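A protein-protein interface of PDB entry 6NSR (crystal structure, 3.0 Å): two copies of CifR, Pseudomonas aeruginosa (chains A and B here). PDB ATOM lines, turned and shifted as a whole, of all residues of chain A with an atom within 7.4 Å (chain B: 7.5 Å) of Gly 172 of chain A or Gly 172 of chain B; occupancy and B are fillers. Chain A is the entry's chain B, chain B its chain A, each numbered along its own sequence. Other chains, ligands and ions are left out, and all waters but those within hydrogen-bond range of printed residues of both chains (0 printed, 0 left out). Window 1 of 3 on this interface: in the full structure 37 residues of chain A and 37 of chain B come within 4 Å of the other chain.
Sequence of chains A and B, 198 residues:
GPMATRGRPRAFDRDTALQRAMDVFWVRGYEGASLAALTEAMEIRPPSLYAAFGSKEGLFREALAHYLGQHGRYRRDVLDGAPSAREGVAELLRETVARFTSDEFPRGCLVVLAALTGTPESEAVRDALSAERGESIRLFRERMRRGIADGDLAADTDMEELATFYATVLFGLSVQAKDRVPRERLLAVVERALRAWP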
ATOM      1  N   PHE A 100     -17.941 -24.621  13.969  1.00  0.00           N
ATOM      2  CA  PHE A 100     -19.007 -23.660  13.719  1.00  0.00           C
ATOM      3  C   PHE A 100     -20.026 -24.203  12.728  1.00  0.00           C
ATOM      4  O   PHE A 100     -21.198 -23.815  12.771  1.00  0.00           O
ATOM      5  CB  PHE A 100     -18.425 -22.350  13.191  1.00  0.00           C
ATOM      6  CG  PHE A 100     -17.864 -21.458  14.258  1.00  0.00           C
ATOM      7  CD1 PHE A 100     -17.883 -21.846  15.587  1.00  0.00           C
ATOM      8  CD2 PHE A 100     -17.330 -20.223  13.933  1.00  0.00           C
ATOM      9  CE1 PHE A 100     -17.369 -21.023  16.570  1.00  0.00           C
ATOM     10  CE2 PHE A 100     -16.817 -19.396  14.911  1.00  0.00           C
ATOM     11  CZ  PHE A 100     -16.838 -19.795  16.231  1.00  0.00           C
ATOM     12  N   VAL A 112     -19.477 -14.708  21.446  1.00  0.00           N
ATOM     13  CA  VAL A 112     -19.785 -13.618  20.527  1.00  0.00           C
ATOM     14  C   VAL A 112     -21.288 -13.404  20.393  1.00  0.00           C
ATOM     15  O   VAL A 112     -21.751 -12.266  20.295  1.00  0.00           O
ATOM     16  CB  VAL A 112     -19.115 -13.877  19.163  1.00  0.00           C
ATOM     17  CG1 VAL A 112     -19.375 -12.726  18.207  1.00  0.00           C
ATOM     18  CG2 VAL A 112     -17.623 -14.098  19.344  1.00  0.00           C
ATOM     19  N   THR A 164      -5.116  -8.917  16.636  1.00  0.00           N
ATOM     20  CA  THR A 164      -6.425  -8.284  16.504  1.00  0.00           C
ATOM     21  C   THR A 164      -7.068  -8.614  15.162  1.00  0.00           C
ATOM     22  O   THR A 164      -8.287  -8.805  15.080  1.00  0.00           O
ATOM     23  CB  THR A 164      -6.309  -6.770  16.692  1.00  0.00           C
ATOM     24  OG1 THR A 164      -5.592  -6.489  17.900  1.00  0.00           O
ATOM     25  CG2 THR A 164      -7.691  -6.141  16.781  1.00  0.00           C
ATOM     26  N   TYR A 166      -6.696 -11.406  13.308  1.00  0.00           N
ATOM     27  CA  TYR A 166      -7.220 -12.767  13.286  1.00  0.00           C
ATOM     28  C   TYR A 166      -8.364 -12.945  14.274  1.00  0.00           C
ATOM     29  O   TYR A 166      -9.260 -13.764  14.042  1.00  0.00           O
ATOM     30  CB  TYR A 166      -6.095 -13.780  13.497  1.00  0.00           C
ATOM     31  CG  TYR A 166      -5.273 -13.986  12.245  1.00  0.00           C
ATOM     32  CD1 TYR A 166      -5.810 -14.634  11.140  1.00  0.00           C
ATOM     33  CD2 TYR A 166      -3.976 -13.500  12.153  1.00  0.00           C
ATOM     34  CE1 TYR A 166      -5.069 -14.812   9.986  1.00  0.00           C
ATOM     35  CE2 TYR A 166      -3.228 -13.672  11.003  1.00  0.00           C
ATOM     36  CZ  TYR A 166      -3.779 -14.328   9.923  1.00  0.00           C
ATOM     37  OH  TYR A 166      -3.036 -14.503   8.778  1.00  0.00           O
ATOM     38  N   ALA A 167      -8.355 -12.187  15.372  1.00  0.00           N
ATOM     39  CA  ALA A 167      -9.503 -12.189  16.270  1.00  0.00           C
ATOM     40  C   ALA A 167     -10.715 -11.550  15.604  1.00  0.00           C
ATOM     41  O   ALA A 167     -11.851 -11.993  15.812  1.00  0.00           O
ATOM     42  CB  ALA A 167      -9.156 -11.471  17.571  1.00  0.00           C
ATOM     43  N   THR A 168     -10.491 -10.504  14.804  1.00  0.00           N
ATOM     44  CA  THR A 168     -11.574  -9.920  14.019  1.00  0.00           C
ATOM     45  C   THR A 168     -12.167 -10.949  13.065  1.00  0.00           C
ATOM     46  O   THR A 168     -13.392 -11.070  12.945  1.00  0.00           O
ATOM     47  CB  THR A 168     -11.057  -8.701  13.255  1.00  0.00           C
ATOM     48  OG1 THR A 168     -10.554  -7.732  14.183  1.00  0.00           O
ATOM     49  CG2 THR A 168     -12.165  -8.076  12.427  1.00  0.00           C
ATOM     50  N   VAL A 169     -11.307 -11.700  12.373  1.00  0.00           N
ATOM     51  CA  VAL A 169     -11.787 -12.746  11.474  1.00  0.00           C
ATOM     52  C   VAL A 169     -12.538 -13.815  12.258  1.00  0.00           C
ATOM     53  O   VAL A 169     -13.552 -14.350  11.796  1.00  0.00           O
ATOM     54  CB  VAL A 169     -10.622 -13.333  10.654  1.00  0.00           C
ATOM     55  CG1 VAL A 169     -11.103 -14.489   9.789  1.00  0.00           C
ATOM     56  CG2 VAL A 169      -9.985 -12.255   9.791  1.00  0.00           C
ATOM     57  N   LEU A 170     -12.059 -14.129  13.465  1.00  0.00           N
ATOM     58  CA  LEU A 170     -12.720 -15.129  14.298  1.00  0.00           C
ATOM     59  C   LEU A 170     -14.128 -14.690  14.680  1.00  0.00           C
ATOM     60  O   LEU A 170     -15.088 -15.460  14.547  1.00  0.00           O
ATOM     61  CB  LEU A 170     -11.876 -15.403  15.543  1.00  0.00           C
ATOM     62  CG  LEU A 170     -12.268 -16.621  16.378  1.00  0.00           C
ATOM     63  CD1 LEU A 170     -11.879 -17.905  15.667  1.00  0.00           C
ATOM     64  CD2 LEU A 170     -11.621 -16.547  17.751  1.00  0.00           C
ATOM     65  N   PHE A 171     -14.270 -13.460  15.185  1.00  0.00           N
ATOM     66  CA  PHE A 171     -15.591 -12.963  15.559  1.00  0.00           C
ATOM     67  C   PHE A 171     -16.514 -12.888  14.349  1.00  0.00           C
ATOM     68  O   PHE A 171     -17.691 -13.260  14.428  1.00  0.00           O
ATOM     69  CB  PHE A 171     -15.476 -11.598  16.236  1.00  0.00           C
ATOM     70  CG  PHE A 171     -14.544 -11.575  17.415  1.00  0.00           C
ATOM     71  CD1 PHE A 171     -14.377 -12.696  18.210  1.00  0.00           C
ATOM     72  CD2 PHE A 171     -13.846 -10.422  17.737  1.00  0.00           C
ATOM     73  CE1 PHE A 171     -13.525 -12.673  19.298  1.00  0.00           C
ATOM     74  CE2 PHE A 171     -12.993 -10.392  18.823  1.00  0.00           C
ATOM     75  CZ  PHE A 171     -12.832 -11.519  19.604  1.00  0.00           C
ATOM     76  N   GLY A 172     -15.992 -12.409  13.217  1.00  0.00           N
ATOM     77  CA  GLY A 172     -16.767 -12.398  11.987  1.00  0.00           C
ATOM     78  C   GLY A 172     -17.199 -13.776  11.532  1.00  0.00           C
ATOM     79  O   GLY A 172     -18.289 -13.935  10.978  1.00  0.00           O
ATOM     80  N   LEU A 173     -16.363 -14.790  11.768  1.00  0.00           N
ATOM     81  CA  LEU A 173     -16.730 -16.158  11.410  1.00  0.00           C
ATOM     82  C   LEU A 173     -17.893 -16.664  12.254  1.00  0.00           C
ATOM     83  O   LEU A 173     -18.760 -17.389  11.750  1.00  0.00           O
ATOM     84  CB  LEU A 173     -15.523 -17.085  11.555  1.00  0.00           C
ATOM     85  CG  LEU A 173     -14.466 -17.015  10.454  1.00  0.00           C
ATOM     86  CD1 LEU A 173     -13.366 -18.031  10.707  1.00  0.00           C
ATOM     87  CD2 LEU A 173     -15.088 -17.221   9.084  1.00  0.00           C
ATOM     88  N   SER A 174     -17.923 -16.308  13.540  1.00  0.00           N
ATOM     89  CA  SER A 174     -19.082 -16.628  14.369  1.00  0.00           C
ATOM     90  C   SER A 174     -20.356 -16.043  13.767  1.00  0.00           C
ATOM     91  O   SER A 174     -21.372 -16.735  13.645  1.00  0.00           O
ATOM     92  CB  SER A 174     -18.860 -16.123  15.794  1.00  0.00           C
ATOM     93  OG  SER A 174     -19.923 -16.511  16.644  1.00  0.00           O
ATOM     94  N   VAL A 175     -20.326 -14.755  13.415  1.00  0.00           N
ATOM     95  CA  VAL A 175     -21.495 -14.109  12.821  1.00  0.00           C
ATOM     96  C   VAL A 175     -21.892 -14.802  11.521  1.00  0.00           C
ATOM     97  O   VAL A 175     -23.081 -15.012  11.249  1.00  0.00           O
ATOM     98  CB  VAL A 175     -21.234 -12.603  12.623  1.00  0.00           C
ATOM     99  CG1 VAL A 175     -22.330 -11.970  11.772  1.00  0.00           C
ATOM    100  CG2 VAL A 175     -21.132 -11.907  13.970  1.00  0.00           C
ATOM    101  N   GLN A 176     -20.904 -15.159  10.693  1.00  0.00           N
ATOM    102  CA  GLN A 176     -21.203 -15.801   9.416  1.00  0.00           C
ATOM    103  C   GLN A 176     -21.776 -17.199   9.613  1.00  0.00           C
ATOM    104  O   GLN A 176     -22.685 -17.612   8.883  1.00  0.00           O
ATOM    105  CB  GLN A 176     -19.949 -15.860   8.541  1.00  0.00           C
ATOM    106  CG  GLN A 176     -19.396 -14.509   8.117  1.00  0.00           C
ATOM    107  CD  GLN A 176     -20.096 -13.933   6.901  1.00  0.00           C
ATOM    108  OE1 GLN A 176     -21.274 -14.197   6.660  1.00  0.00           O
ATOM    109  NE2 GLN A 176     -19.367 -13.141   6.124  1.00  0.00           N
ATOM    110  N   ALA A 177     -21.249 -17.945  10.589  1.00  0.00           N
ATOM    111  CA  ALA A 177     -21.801 -19.262  10.890  1.00  0.00           C
ATOM    112  C   ALA A 177     -23.245 -19.176  11.365  1.00  0.00           C
ATOM    113  O   ALA A 177     -24.044 -20.076  11.084  1.00  0.00           O
ATOM    114  CB  ALA A 177     -20.934 -19.962  11.935  1.00  0.00           C
ATOM    115  N   LYS A 178     -23.599 -18.104  12.079  1.00  0.00           N
ATOM    116  CA  LYS A 178     -24.996 -17.891  12.444  1.00  0.00           C
ATOM    117  C   LYS A 178     -25.866 -17.670  11.215  1.00  0.00           C
ATOM    118  O   LYS A 178     -27.040 -18.055  11.209  1.00  0.00           O
ATOM    119  CB  LYS A 178     -25.114 -16.705  13.403  1.00  0.00           C
ATOM    120  CG  LYS A 178     -26.422 -16.658  14.172  1.00  0.00           C
ATOM    121  CD  LYS A 178     -26.557 -17.868  15.081  1.00  0.00           C
ATOM    122  CE  LYS A 178     -27.818 -17.797  15.924  1.00  0.00           C
ATOM    123  NZ  LYS A 178     -27.871 -18.905  16.920  1.00  0.00           N
ATOM    124  N   LEU A 186     -16.536 -20.689   4.438  1.00  0.00           N
ATOM    125  CA  LEU A 186     -15.803 -20.237   5.615  1.00  0.00           C
ATOM    126  C   LEU A 186     -14.361 -20.723   5.603  1.00  0.00           C
ATOM    127  O   LEU A 186     -13.466 -20.011   6.068  1.00  0.00           O
ATOM    128  CB  LEU A 186     -16.512 -20.691   6.889  1.00  0.00           C
ATOM    129  CG  LEU A 186     -17.895 -20.079   7.115  1.00  0.00           C
ATOM    130  CD1 LEU A 186     -18.491 -20.567   8.425  1.00  0.00           C
ATOM    131  CD2 LEU A 186     -17.823 -18.561   7.078  1.00  0.00           C
ATOM    132  N   VAL A 189     -12.602 -18.416   3.461  1.00  0.00           N
ATOM    133  CA  VAL A 189     -12.359 -17.181   4.201  1.00  0.00           C
ATOM    134  C   VAL A 189     -11.119 -17.317   5.075  1.00  0.00           C
ATOM    135  O   VAL A 189     -10.300 -16.394   5.163  1.00  0.00           O
ATOM    136  CB  VAL A 189     -13.606 -16.795   5.019  1.00  0.00           C
ATOM    137  CG1 VAL A 189     -13.281 -15.681   6.005  1.00  0.00           C
ATOM    138  CG2 VAL A 189     -14.737 -16.384   4.093  1.00  0.00           C
ATOM    139  N   PHE B 100     -17.491   3.576  13.162  1.00  0.00           N
ATOM    140  CA  PHE B 100     -17.598   2.685  14.313  1.00  0.00           C
ATOM    141  C   PHE B 100     -16.907   3.268  15.535  1.00  0.00           C
ATOM    142  O   PHE B 100     -17.321   3.003  16.669  1.00  0.00           O
ATOM    143  CB  PHE B 100     -16.994   1.318  13.983  1.00  0.00           C
ATOM    144  CG  PHE B 100     -17.871   0.449  13.127  1.00  0.00           C
ATOM    145  CD1 PHE B 100     -19.129   0.874  12.734  1.00  0.00           C
ATOM    146  CD2 PHE B 100     -17.437  -0.803  12.725  1.00  0.00           C
ATOM    147  CE1 PHE B 100     -19.931   0.069  11.950  1.00  0.00           C
ATOM    148  CE2 PHE B 100     -18.238  -1.612  11.942  1.00  0.00           C
ATOM    149  CZ  PHE B 100     -19.486  -1.176  11.556  1.00  0.00           C
ATOM    150  N   VAL B 112     -25.515  -5.658  12.682  1.00  0.00           N
ATOM    151  CA  VAL B 112     -24.783  -6.780  13.260  1.00  0.00           C
ATOM    152  C   VAL B 112     -25.090  -6.953  14.743  1.00  0.00           C
ATOM    153  O   VAL B 112     -25.218  -8.080  15.225  1.00  0.00           O
ATOM    154  CB  VAL B 112     -23.271  -6.622  13.001  1.00  0.00           C
ATOM    155  CG1 VAL B 112     -22.505  -7.824  13.537  1.00  0.00           C
ATOM    156  CG2 VAL B 112     -23.001  -6.423  11.515  1.00  0.00           C
ATOM    157  N   THR B 164     -17.215 -12.392   0.727  1.00  0.00           N
ATOM    158  CA  THR B 164     -17.479 -13.008   2.023  1.00  0.00           C
ATOM    159  C   THR B 164     -16.354 -12.724   3.011  1.00  0.00           C
ATOM    160  O   THR B 164     -16.606 -12.492   4.200  1.00  0.00           O
ATOM    161  CB  THR B 164     -17.699 -14.511   1.859  1.00  0.00           C
ATOM    162  OG1 THR B 164     -18.753 -14.741   0.916  1.00  0.00           O
ATOM    163  CG2 THR B 164     -18.071 -15.150   3.189  1.00  0.00           C
ATOM    164  N   TYR B 166     -14.285 -10.054   3.111  1.00  0.00           N
ATOM    165  CA  TYR B 166     -14.306  -8.673   3.577  1.00  0.00           C
ATOM    166  C   TYR B 166     -15.570  -8.367   4.369  1.00  0.00           C
ATOM    167  O   TYR B 166     -15.556  -7.492   5.242  1.00  0.00           O
ATOM    168  CB  TYR B 166     -14.080  -7.706   2.414  1.00  0.00           C
ATOM    169  CG  TYR B 166     -12.624  -7.627   2.011  1.00  0.00           C
ATOM    170  CD1 TYR B 166     -11.679  -7.065   2.862  1.00  0.00           C
ATOM    171  CD2 TYR B 166     -12.190  -8.139   0.796  1.00  0.00           C
ATOM    172  CE1 TYR B 166     -10.343  -7.001   2.506  1.00  0.00           C
ATOM    173  CE2 TYR B 166     -10.858  -8.080   0.431  1.00  0.00           C
ATOM    174  CZ  TYR B 166      -9.938  -7.509   1.289  1.00  0.00           C
ATOM    175  OH  TYR B 166      -8.611  -7.448   0.928  1.00  0.00           O
ATOM    176  N   ALA B 167     -16.667  -9.068   4.080  1.00  0.00           N
ATOM    177  CA  ALA B 167     -17.847  -8.952   4.927  1.00  0.00           C
ATOM    178  C   ALA B 167     -17.587  -9.573   6.294  1.00  0.00           C
ATOM    179  O   ALA B 167     -18.065  -9.064   7.315  1.00  0.00           O
ATOM    180  CB  ALA B 167     -19.054  -9.600   4.252  1.00  0.00           C
ATOM    181  N   THR B 168     -16.822 -10.668   6.330  1.00  0.00           N
ATOM    182  CA  THR B 168     -16.410 -11.248   7.604  1.00  0.00           C
ATOM    183  C   THR B 168     -15.587 -10.254   8.412  1.00  0.00           C
ATOM    184  O   THR B 168     -15.786 -10.112   9.624  1.00  0.00           O
ATOM    185  CB  THR B 168     -15.617 -12.533   7.366  1.00  0.00           C
ATOM    186  OG1 THR B 168     -16.408 -13.458   6.609  1.00  0.00           O
ATOM    187  CG2 THR B 168     -15.234 -13.175   8.690  1.00  0.00           C
ATOM    188  N   VAL B 169     -14.646  -9.566   7.760  1.00  0.00           N
ATOM    189  CA  VAL B 169     -13.858  -8.547   8.448  1.00  0.00           C
ATOM    190  C   VAL B 169     -14.763  -7.423   8.939  1.00  0.00           C
ATOM    191  O   VAL B 169     -14.551  -6.861  10.020  1.00  0.00           O
ATOM    192  CB  VAL B 169     -12.729  -8.031   7.536  1.00  0.00           C
ATOM    193  CG1 VAL B 169     -11.923  -6.951   8.239  1.00  0.00           C
ATOM    194  CG2 VAL B 169     -11.828  -9.177   7.108  1.00  0.00           C
ATOM    195  N   LEU B 170     -15.802  -7.098   8.164  1.00  0.00           N
ATOM    196  CA  LEU B 170     -16.731  -6.042   8.555  1.00  0.00           C
ATOM    197  C   LEU B 170     -17.497  -6.421   9.814  1.00  0.00           C
ATOM    198  O   LEU B 170     -17.581  -5.632  10.763  1.00  0.00           O
ATOM    199  CB  LEU B 170     -17.707  -5.765   7.412  1.00  0.00           C
ATOM    200  CG  LEU B 170     -18.287  -4.356   7.266  1.00  0.00           C
ATOM    201  CD1 LEU B 170     -17.253  -3.358   6.807  1.00  0.00           C
ATOM    202  CD2 LEU B 170     -19.453  -4.399   6.294  1.00  0.00           C
ATOM    203  N   PHE B 171     -18.079  -7.622   9.831  1.00  0.00           N
ATOM    204  CA  PHE B 171     -18.810  -8.074  11.010  1.00  0.00           C
ATOM    205  C   PHE B 171     -17.899  -8.152  12.229  1.00  0.00           C
ATOM    206  O   PHE B 171     -18.283  -7.740  13.329  1.00  0.00           O
ATOM    207  CB  PHE B 171     -19.467  -9.426  10.727  1.00  0.00           C
ATOM    208  CG  PHE B 171     -20.311  -9.446   9.478  1.00  0.00           C
ATOM    209  CD1 PHE B 171     -20.972  -8.304   9.047  1.00  0.00           C
ATOM    210  CD2 PHE B 171     -20.440 -10.607   8.733  1.00  0.00           C
ATOM    211  CE1 PHE B 171     -21.745  -8.323   7.899  1.00  0.00           C
ATOM    212  CE2 PHE B 171     -21.213 -10.630   7.584  1.00  0.00           C
ATOM    213  CZ  PHE B 171     -21.865  -9.485   7.169  1.00  0.00           C
ATOM    214  N   GLY B 172     -16.683  -8.672  12.050  1.00  0.00           N
ATOM    215  CA  GLY B 172     -15.715  -8.676  13.134  1.00  0.00           C
ATOM    216  C   GLY B 172     -15.380  -7.290  13.650  1.00  0.00           C
ATOM    217  O   GLY B 172     -15.166  -7.105  14.850  1.00  0.00           O
ATOM    218  N   LEU B 173     -15.358  -6.297  12.760  1.00  0.00           N
ATOM    219  CA  LEU B 173     -15.085  -4.923  13.174  1.00  0.00           C
ATOM    220  C   LEU B 173     -16.205  -4.355  14.040  1.00  0.00           C
ATOM    221  O   LEU B 173     -15.939  -3.603  14.984  1.00  0.00           O
ATOM    222  CB  LEU B 173     -14.822  -4.043  11.952  1.00  0.00           C
ATOM    223  CG  LEU B 173     -13.439  -4.218  11.320  1.00  0.00           C
ATOM    224  CD1 LEU B 173     -13.276  -3.312  10.113  1.00  0.00           C
ATOM    225  CD2 LEU B 173     -12.338  -3.967  12.342  1.00  0.00           C
ATOM    226  N   SER B 174     -17.462  -4.687  13.731  1.00  0.00           N
ATOM    227  CA  SER B 174     -18.557  -4.320  14.625  1.00  0.00           C
ATOM    228  C   SER B 174     -18.320  -4.859  16.030  1.00  0.00           C
ATOM    229  O   SER B 174     -18.441  -4.125  17.017  1.00  0.00           O
ATOM    230  CB  SER B 174     -19.888  -4.829  14.071  1.00  0.00           C
ATOM    231  OG  SER B 174     -20.334  -4.024  12.996  1.00  0.00           O
ATOM    232  N   VAL B 175     -17.992  -6.148  16.142  1.00  0.00           N
ATOM    233  CA  VAL B 175     -17.758  -6.737  17.457  1.00  0.00           C
ATOM    234  C   VAL B 175     -16.596  -6.037  18.155  1.00  0.00           C
ATOM    235  O   VAL B 175     -16.664  -5.735  19.353  1.00  0.00           O
ATOM    236  CB  VAL B 175     -17.542  -8.258  17.339  1.00  0.00           C
ATOM    237  CG1 VAL B 175     -16.990  -8.822  18.636  1.00  0.00           C
ATOM    238  CG2 VAL B 175     -18.844  -8.947  16.973  1.00  0.00           C
ATOM    239  N   GLN B 176     -15.518  -5.758  17.416  1.00  0.00           N
ATOM    240  CA  GLN B 176     -14.359  -5.114  18.027  1.00  0.00           C
ATOM    241  C   GLN B 176     -14.673  -3.681  18.442  1.00  0.00           C
ATOM    242  O   GLN B 176     -14.216  -3.220  19.495  1.00  0.00           O
ATOM    243  CB  GLN B 176     -13.169  -5.138  17.067  1.00  0.00           C
ATOM    244  CG  GLN B 176     -12.686  -6.526  16.674  1.00  0.00           C
ATOM    245  CD  GLN B 176     -11.753  -7.145  17.697  1.00  0.00           C
ATOM    246  OE1 GLN B 176     -11.853  -6.877  18.894  1.00  0.00           O
ATOM    247  NE2 GLN B 176     -10.829  -7.973  17.224  1.00  0.00           N
ATOM    248  N   ALA B 177     -15.448  -2.959  17.625  1.00  0.00           N
ATOM    249  CA  ALA B 177     -15.813  -1.592  17.983  1.00  0.00           C
ATOM    250  C   ALA B 177     -16.728  -1.553  19.199  1.00  0.00           C
ATOM    251  O   ALA B 177     -16.647  -0.617  20.003  1.00  0.00           O
ATOM    252  CB  ALA B 177     -16.471  -0.893  16.794  1.00  0.00           C
ATOM    253  N   LYS B 178     -17.602  -2.552  19.347  1.00  0.00           N
ATOM    254  CA  LYS B 178     -18.399  -2.669  20.562  1.00  0.00           C
ATOM    255  C   LYS B 178     -17.515  -2.875  21.784  1.00  0.00           C
ATOM    256  O   LYS B 178     -17.849  -2.412  22.880  1.00  0.00           O
ATOM    257  CB  LYS B 178     -19.400  -3.815  20.426  1.00  0.00           C
ATOM    258  CG  LYS B 178     -20.477  -3.834  21.496  1.00  0.00           C
ATOM    259  CD  LYS B 178     -21.370  -2.609  21.394  1.00  0.00           C
ATOM    260  CE  LYS B 178     -22.564  -2.713  22.328  1.00  0.00           C
ATOM    261  NZ  LYS B 178     -23.523  -1.590  22.130  1.00  0.00           N
ATOM    262  N   ASP B 179     -16.389  -3.569  21.616  1.00  0.00           N
ATOM    263  CA  ASP B 179     -15.430  -3.807  22.687  1.00  0.00           C
ATOM    264  C   ASP B 179     -14.506  -2.618  22.929  1.00  0.00           C
ATOM    265  O   ASP B 179     -13.574  -2.732  23.735  1.00  0.00           O
ATOM    266  CB  ASP B 179     -14.608  -5.064  22.389  1.00  0.00           C
ATOM    267  CG  ASP B 179     -15.417  -6.339  22.542  1.00  0.00           C
ATOM    268  OD1 ASP B 179     -16.551  -6.270  23.064  1.00  0.00           O
ATOM    269  OD2 ASP B 179     -14.919  -7.413  22.137  1.00  0.00           O
ATOM    270  N   LEU B 186      -7.901  -0.593  14.909  1.00  0.00           N
ATOM    271  CA  LEU B 186      -8.884  -1.083  13.946  1.00  0.00           C
ATOM    272  C   LEU B 186      -8.502  -0.701  12.522  1.00  0.00           C
ATOM    273  O   LEU B 186      -8.714  -1.481  11.586  1.00  0.00           O
ATOM    274  CB  LEU B 186     -10.281  -0.573  14.299  1.00  0.00           C
ATOM    275  CG  LEU B 186     -10.896  -1.148  15.575  1.00  0.00           C
ATOM    276  CD1 LEU B 186     -12.307  -0.624  15.783  1.00  0.00           C
ATOM    277  CD2 LEU B 186     -10.894  -2.666  15.518  1.00  0.00           C
ATOM    278  N   VAL B 189      -5.982  -3.110  11.485  1.00  0.00           N
ATOM    279  CA  VAL B 189      -6.637  -4.348  11.067  1.00  0.00           C
ATOM    280  C   VAL B 189      -7.149  -4.229   9.637  1.00  0.00           C
ATOM    281  O   VAL B 189      -7.070  -5.184   8.854  1.00  0.00           O
ATOM    282  CB  VAL B 189      -7.756  -4.721  12.059  1.00  0.00           C
ATOM    283  CG1 VAL B 189      -8.620  -5.845  11.506  1.00  0.00           C
ATOM    284  CG2 VAL B 189      -7.159  -5.116  13.395  1.00  0.00           C
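Among the printed residues, merely in contact across the chains: Thr 168 of chain A with Gly 172 of chain B, Gly 172 of chain A with Thr 168 of chain B, Gln 176 of chain A with Phe 171 of chain B, Thr 164 of chain A with Val 189 of chain B, Thr 168 of chain A with Val 169 of chain B, Phe 171 of chain A with Gln 176 of chain B, Phe 171 of chain A with Val 175 of chain B, Leu 173 of chain A with Thr 168 of chain B, Val 189 of chain A with Thr 164 of chain B, Thr 168 of chain A with Leu 173 of chain B, Val 169 of chain A with Thr 168 of chain B, Gly 172 of chain A with Gly 172 of chain B, Thr 168 of chain A with Val 189 of chain B, Val 175 of chain A with Phe 171 of chain B, Val 189 of chain A with Thr 168 of chain B, Ala 167 of chain A with Gln 176 of chain B and Gln 176 of chain A with Ala 167 of chain B.
Hydrophobic or aromatic side chains of chain B within 4 Å of the printed part of chain A: Phe 171, Val 175 and Val 189.
Along chain B the printed residues that touch a printed residue of chain A span positions 164 to 189.
Printed residues of chain A that touch a printed residue of chain B: Thr 164, Ala 167, Thr 168, Val 169, Phe 171, Gly 172, Leu 173, Val 175, Gln 176 and Val 189.
Among the printed residues, 21 pairs touch across the chains.
Gly 172 of chain A touches just these residues of chain B: Thr 168 (3.4 Å) and Gly 172 (3.7 Å).
Gly 172 of chain B touches just these residues of chain A: Thr 168 (3.3 Å) and Gly 172 (3.7 Å).
Printed residues of chain B within 4 Å of Val 189 of chain A: Thr 164 and Thr 168.
Of the printed residues of chain A, Leu 173 of chain B touches Thr 168 (3.7 Å).
Printed residues of chain B within 4 Å of Leu 173 of chain A: Thr 168.
Phe 100 of chain B touches none of the printed residues of chain A.
The nearest residue of chain A that does not touch Gly 172 of chain B is Phe 171 of chain A (4.3 Å).
NE2 of Gln 176 of chain A sits at hydrogen-bond distance from O of Thr 164 of chain B.
The side-chain amide nitrogen (NE2) of Gln 176 of chain A is in hydrogen-bond range of the side-chain hydroxyl (OG1) of Thr 168 of chain B, 3.0 Å away.
The backbone carbonyl oxygen (O) of Thr 164 of chain A is in hydrogen-bond range of the side-chain amide nitrogen (NE2) of Gln 176 of chain B (3.4 Å).
NE2 of Gln 176 of chain B is in hydrogen-bond range of OG1 of Thr 168 of chain A, 3.1 Å away.
The backbone carbonyl oxygen of Thr 164 of chain B is in hydrogen-bond range of the side-chain hydroxyl of Thr 168 of chain B (2.6 Å).
O of Thr 164 of chain A lies within hydrogen-bond range of OG1 of Thr 168 of chain A (2.7 Å).
Thr 164 of chain A touches Val 189 of chain B, and with the chains exchanged Val 189 of chain A touches Thr 164 of chain B.
Thr 168 of chain A touches Gln 176 of chain B, and with the chains exchanged Gln 176 of chain A touches Thr 168 of chain B.
Phe 171 of chain A touches Val 175 of chain B, and with the chains exchanged Val 175 of chain A touches Phe 171 of chain B.
Gly 172 of chain B touches its own counterpart, Gly 172 of chain A.
Of the 21 pairs that touch across the chains among the printed residues, 21 have their exchanged pair printed and touching as well.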
